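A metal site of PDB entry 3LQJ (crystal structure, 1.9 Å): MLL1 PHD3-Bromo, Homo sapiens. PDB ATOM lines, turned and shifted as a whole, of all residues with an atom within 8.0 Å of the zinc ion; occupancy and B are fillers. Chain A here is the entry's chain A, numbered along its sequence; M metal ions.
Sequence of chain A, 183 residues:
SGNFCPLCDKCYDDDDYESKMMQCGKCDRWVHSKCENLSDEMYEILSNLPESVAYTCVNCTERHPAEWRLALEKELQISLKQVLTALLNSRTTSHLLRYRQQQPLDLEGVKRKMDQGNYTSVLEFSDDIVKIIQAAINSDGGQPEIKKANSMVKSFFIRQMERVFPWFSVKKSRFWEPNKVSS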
ATOM      1  N   PHE A   4     -19.161  -2.453  30.455  1.00  0.00           N
ATOM      2  CA  PHE A   4     -18.713  -1.423  29.544  1.00  0.00           C
ATOM      3  C   PHE A   4     -19.178  -1.807  28.134  1.00  0.00           C
ATOM      4  O   PHE A   4     -19.155  -2.982  27.770  1.00  0.00           O
ATOM      5  CB  PHE A   4     -17.185  -1.244  29.602  1.00  0.00           C
ATOM      6  CG  PHE A   4     -16.395  -2.445  29.132  1.00  0.00           C
ATOM      7  CD1 PHE A   4     -16.012  -2.569  27.798  1.00  0.00           C
ATOM      8  CD2 PHE A   4     -16.028  -3.441  30.031  1.00  0.00           C
ATOM      9  CE1 PHE A   4     -15.256  -3.668  27.369  1.00  0.00           C
ATOM     10  CE2 PHE A   4     -15.268  -4.538  29.612  1.00  0.00           C
ATOM     11  CZ  PHE A   4     -14.883  -4.643  28.274  1.00  0.00           C
ATOM     12  N   CYS A   5     -19.627  -0.817  27.389  1.00  0.00           N
ATOM     13  CA  CYS A   5     -20.092  -1.020  26.020  1.00  0.00           C
ATOM     14  C   CYS A   5     -18.890  -1.405  25.165  1.00  0.00           C
ATOM     15  O   CYS A   5     -17.867  -0.737  25.174  1.00  0.00           O
ATOM     16  CB  CYS A   5     -20.727   0.251  25.488  1.00  0.00           C
ATOM     17  SG  CYS A   5     -21.221   0.172  23.742  1.00  0.00           S
ATOM     18  N   PRO A   6     -19.008  -2.499  24.391  1.00  0.00           N
ATOM     19  CA  PRO A   6     -17.841  -2.871  23.589  1.00  0.00           C
ATOM     20  C   PRO A   6     -17.471  -1.885  22.475  1.00  0.00           C
ATOM     21  O   PRO A   6     -16.293  -1.744  22.132  1.00  0.00           O
ATOM     22  CB  PRO A   6     -18.224  -4.244  23.041  1.00  0.00           C
ATOM     23  CG  PRO A   6     -19.728  -4.193  22.967  1.00  0.00           C
ATOM     24  CD  PRO A   6     -20.102  -3.468  24.243  1.00  0.00           C
ATOM     25  N   LEU A   7     -18.466  -1.184  21.942  1.00  0.00           N
ATOM     26  CA  LEU A   7     -18.240  -0.261  20.841  1.00  0.00           C
ATOM     27  C   LEU A   7     -17.591   1.080  21.201  1.00  0.00           C
ATOM     28  O   LEU A   7     -16.702   1.551  20.485  1.00  0.00           O
ATOM     29  CB  LEU A   7     -19.573  -0.023  20.106  1.00  0.00           C
ATOM     30  CG  LEU A   7     -20.227  -1.282  19.505  1.00  0.00           C
ATOM     31  CD1 LEU A   7     -21.609  -0.943  18.973  1.00  0.00           C
ATOM     32  CD2 LEU A   7     -19.357  -1.836  18.376  1.00  0.00           C
ATOM     33  N   CYS A   8     -18.026   1.701  22.298  1.00  0.00           N
ATOM     34  CA  CYS A   8     -17.466   2.981  22.715  1.00  0.00           C
ATOM     35  C   CYS A   8     -16.455   2.783  23.834  1.00  0.00           C
ATOM     36  O   CYS A   8     -15.683   3.684  24.147  1.00  0.00           O
ATOM     37  CB  CYS A   8     -18.586   3.914  23.187  1.00  0.00           C
ATOM     38  SG  CYS A   8     -19.340   3.459  24.768  1.00  0.00           S
ATOM     39  N   ASP A   9     -16.486   1.590  24.431  1.00  0.00           N
ATOM     40  CA  ASP A   9     -15.575   1.202  25.500  1.00  0.00           C
ATOM     41  C   ASP A   9     -15.855   1.829  26.864  1.00  0.00           C
ATOM     42  O   ASP A   9     -15.123   1.576  27.825  1.00  0.00           O
ATOM     43  CB  ASP A   9     -14.128   1.522  25.069  1.00  0.00           C
ATOM     44  CG  ASP A   9     -13.097   0.663  25.780  1.00  0.00           C
ATOM     45  OD1 ASP A   9     -13.241  -0.582  25.743  1.00  0.00           O
ATOM     46  OD2 ASP A   9     -12.145   1.219  26.355  1.00  0.00           O
ATOM     47  N   LYS A  10     -16.910   2.640  26.950  1.00  0.00           N
ATOM     48  CA  LYS A  10     -17.269   3.317  28.195  1.00  0.00           C
ATOM     49  C   LYS A  10     -18.124   2.471  29.129  1.00  0.00           C
ATOM     50  O   LYS A  10     -18.885   1.591  28.703  1.00  0.00           O
ATOM     51  CB  LYS A  10     -18.012   4.618  27.885  1.00  0.00           C
ATOM     52  CG  LYS A  10     -17.261   5.524  26.925  1.00  0.00           C
ATOM     53  CD  LYS A  10     -17.952   6.860  26.805  1.00  0.00           C
ATOM     54  CE  LYS A  10     -17.136   7.827  25.953  1.00  0.00           C
ATOM     55  NZ  LYS A  10     -17.753   9.177  25.967  1.00  0.00           N
ATOM     56  N   CYS A  11     -17.995   2.753  30.427  1.00  0.00           N
ATOM     57  CA  CYS A  11     -18.712   2.064  31.486  1.00  0.00           C
ATOM     58  C   CYS A  11     -20.195   2.394  31.507  1.00  0.00           C
ATOM     59  O   CYS A  11     -20.621   3.434  31.023  1.00  0.00           O
ATOM     60  CB  CYS A  11     -18.063   2.457  32.836  1.00  0.00           C
ATOM     61  SG  CYS A  11     -18.890   1.877  34.350  1.00  0.00           S
ATOM     62  N   TYR A  12     -21.001   1.475  32.043  1.00  0.00           N
ATOM     63  CA  TYR A  12     -22.434   1.705  32.177  1.00  0.00           C
ATOM     64  C   TYR A  12     -22.884   1.122  33.507  1.00  0.00           C
ATOM     65  O   TYR A  12     -22.298   0.145  33.995  1.00  0.00           O
ATOM     66  CB  TYR A  12     -23.223   1.113  31.004  1.00  0.00           C
ATOM     67  CG  TYR A  12     -23.168  -0.397  30.863  1.00  0.00           C
ATOM     68  CD1 TYR A  12     -23.848  -1.233  31.739  1.00  0.00           C
ATOM     69  CD2 TYR A  12     -22.447  -0.981  29.818  1.00  0.00           C
ATOM     70  CE1 TYR A  12     -23.806  -2.629  31.598  1.00  0.00           C
ATOM     71  CE2 TYR A  12     -22.397  -2.370  29.663  1.00  0.00           C
ATOM     72  CZ  TYR A  12     -23.082  -3.184  30.549  1.00  0.00           C
ATOM     73  OH  TYR A  12     -23.029  -4.553  30.391  1.00  0.00           O
ATOM     74  N   LYS A  20     -30.318   4.073  26.880  1.00  0.00           N
ATOM     75  CA  LYS A  20     -30.845   3.371  25.722  1.00  0.00           C
ATOM     76  C   LYS A  20     -29.793   2.363  25.313  1.00  0.00           C
ATOM     77  O   LYS A  20     -28.799   2.711  24.663  1.00  0.00           O
ATOM     78  CB  LYS A  20     -31.136   4.336  24.569  1.00  0.00           C
ATOM     79  CG  LYS A  20     -32.363   5.214  24.818  1.00  0.00           C
ATOM     80  CD  LYS A  20     -32.779   5.998  23.592  1.00  0.00           C
ATOM     81  CE  LYS A  20     -34.098   6.713  23.838  1.00  0.00           C
ATOM     82  NZ  LYS A  20     -34.023   7.571  25.058  1.00  0.00           N
ATOM     83  N   MET A  21     -29.993   1.119  25.727  1.00  0.00           N
ATOM     84  CA  MET A  21     -29.059   0.050  25.417  1.00  0.00           C
ATOM     85  C   MET A  21     -29.808  -1.216  25.069  1.00  0.00           C
ATOM     86  O   MET A  21     -30.953  -1.412  25.483  1.00  0.00           O
ATOM     87  CB  MET A  21     -28.160  -0.240  26.637  1.00  0.00           C
ATOM     88  CG  MET A  21     -27.486   0.973  27.227  1.00  0.00           C
ATOM     89  SD  MET A  21     -26.298   0.546  28.498  1.00  0.00           S
ATOM     90  CE  MET A  21     -24.926  -0.040  27.477  1.00  0.00           C
ATOM     91  N   TRP A  30     -24.541  -5.520  27.435  1.00  0.00           N
ATOM     92  CA  TRP A  30     -25.308  -4.402  26.934  1.00  0.00           C
ATOM     93  C   TRP A  30     -24.508  -3.507  26.001  1.00  0.00           C
ATOM     94  O   TRP A  30     -23.292  -3.347  26.161  1.00  0.00           O
ATOM     95  CB  TRP A  30     -25.850  -3.585  28.092  1.00  0.00           C
ATOM     96  CG  TRP A  30     -26.885  -4.329  28.901  1.00  0.00           C
ATOM     97  CD1 TRP A  30     -26.660  -5.206  29.926  1.00  0.00           C
ATOM     98  CD2 TRP A  30     -28.297  -4.287  28.714  1.00  0.00           C
ATOM     99  NE1 TRP A  30     -27.851  -5.703  30.393  1.00  0.00           N
ATOM    100  CE2 TRP A  30     -28.876  -5.163  29.669  1.00  0.00           C
ATOM    101  CE3 TRP A  30     -29.144  -3.590  27.828  1.00  0.00           C
ATOM    102  CZ2 TRP A  30     -30.253  -5.353  29.765  1.00  0.00           C
ATOM    103  CZ3 TRP A  30     -30.509  -3.781  27.931  1.00  0.00           C
ATOM    104  CH2 TRP A  30     -31.053  -4.659  28.896  1.00  0.00           C
ATOM    105  N   VAL A  31     -25.191  -2.960  25.007  1.00  0.00           N
ATOM    106  CA  VAL A  31     -24.571  -2.095  24.019  1.00  0.00           C
ATOM    107  C   VAL A  31     -25.441  -0.859  23.780  1.00  0.00           C
ATOM    108  O   VAL A  31     -26.664  -0.965  23.636  1.00  0.00           O
ATOM    109  CB  VAL A  31     -24.367  -2.851  22.686  1.00  0.00           C
ATOM    110  CG1 VAL A  31     -23.619  -1.961  21.686  1.00  0.00           C
ATOM    111  CG2 VAL A  31     -23.604  -4.165  22.928  1.00  0.00           C
ATOM    112  N   HIS A  32     -24.816   0.310  23.767  1.00  0.00           N
ATOM    113  CA  HIS A  32     -25.540   1.572  23.541  1.00  0.00           C
ATOM    114  C   HIS A  32     -26.198   1.615  22.170  1.00  0.00           C
ATOM    115  O   HIS A  32     -25.602   1.234  21.160  1.00  0.00           O
ATOM    116  CB  HIS A  32     -24.575   2.769  23.627  1.00  0.00           C
ATOM    117  CG  HIS A  32     -24.070   3.072  25.003  1.00  0.00           C
ATOM    118  ND1 HIS A  32     -22.729   3.187  25.288  1.00  0.00           N
ATOM    119  CD2 HIS A  32     -24.726   3.331  26.164  1.00  0.00           C
ATOM    120  CE1 HIS A  32     -22.579   3.504  26.564  1.00  0.00           C
ATOM    121  NE2 HIS A  32     -23.773   3.592  27.116  1.00  0.00           N
ATOM    122  N   SER A  33     -27.434   2.112  22.143  1.00  0.00           N
ATOM    123  CA  SER A  33     -28.201   2.262  20.910  1.00  0.00           C
ATOM    124  C   SER A  33     -27.447   3.202  19.975  1.00  0.00           C
ATOM    125  O   SER A  33     -27.310   2.936  18.781  1.00  0.00           O
ATOM    126  CB  SER A  33     -29.581   2.845  21.236  1.00  0.00           C
ATOM    127  OG  SER A  33     -30.298   3.150  20.051  1.00  0.00           O
ATOM    128  N   LYS A  34     -26.951   4.306  20.521  1.00  0.00           N
ATOM    129  CA  LYS A  34     -26.231   5.294  19.729  1.00  0.00           C
ATOM    130  C   LYS A  34     -24.918   4.731  19.168  1.00  0.00           C
ATOM    131  O   LYS A  34     -24.443   5.197  18.130  1.00  0.00           O
ATOM    132  CB  LYS A  34     -25.944   6.551  20.554  1.00  0.00           C
ATOM    133  CG  LYS A  34     -24.838   6.407  21.572  1.00  0.00           C
ATOM    134  CD  LYS A  34     -24.723   7.668  22.420  1.00  0.00           C
ATOM    135  CE  LYS A  34     -23.527   7.624  23.365  1.00  0.00           C
ATOM    136  NZ  LYS A  34     -22.240   7.847  22.669  1.00  0.00           N
ATOM    137  N   CYS A  35     -24.319   3.753  19.842  1.00  0.00           N
ATOM    138  CA  CYS A  35     -23.061   3.196  19.341  1.00  0.00           C
ATOM    139  C   CYS A  35     -23.264   2.277  18.149  1.00  0.00           C
ATOM    140  O   CYS A  35     -22.328   2.021  17.394  1.00  0.00           O
ATOM    141  CB  CYS A  35     -22.313   2.465  20.443  1.00  0.00           C
ATOM    142  SG  CYS A  35     -21.731   3.641  21.661  1.00  0.00           S
ATOM    143  N   GLU A  36     -24.496   1.799  17.971  1.00  0.00           N
ATOM    144  CA  GLU A  36     -24.830   0.955  16.832  1.00  0.00           C
ATOM    145  C   GLU A  36     -25.431   1.869  15.765  1.00  0.00           C
ATOM    146  O   GLU A  36     -26.024   1.398  14.788  1.00  0.00           O
ATOM    147  CB  GLU A  36     -25.858  -0.121  17.248  1.00  0.00           C
ATOM    148  CG  GLU A  36     -25.291  -1.263  18.081  1.00  0.00           C
ATOM    149  CD  GLU A  36     -24.468  -2.243  17.244  1.00  0.00           C
ATOM    150  OE1 GLU A  36     -24.084  -1.904  16.114  1.00  0.00           O
ATOM    151  OE2 GLU A  36     -24.207  -3.353  17.747  1.00  0.00           O
HETATM  152 ZN    ZN M   1     -21.359   2.532  23.662  1.00  0.00          ZN
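The side-chain sulfur (SG) of Cys 5 sits close to the backbone NH (N) of Leu 7, at 3.6 Å. N of Cys 5 sits at hydrogen-bond distance from O of Lys 10, 2.8 Å away. SG of Cys 8 lies close to N of Lys 10, at 3.4 Å.
Four residues have an atom within 4 Å of the zinc ion: Cys 5, Cys 8, His 32 and Cys 35. The nearest printed residue that does not touch the zinc ion is Leu 7 (4.7 Å).
The zinc ion is bound by a ring nitrogen (ND1) of His 32 (2.2 Å), the side-chain sulfur (SG) of Cys 35 (2.3 Å), the side-chain sulfur (SG) of Cys 5 (2.4 Å) and the side-chain sulfur (SG) of Cys 8 (2.5 Å). The zinc ion has four donor atoms within binding distance.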
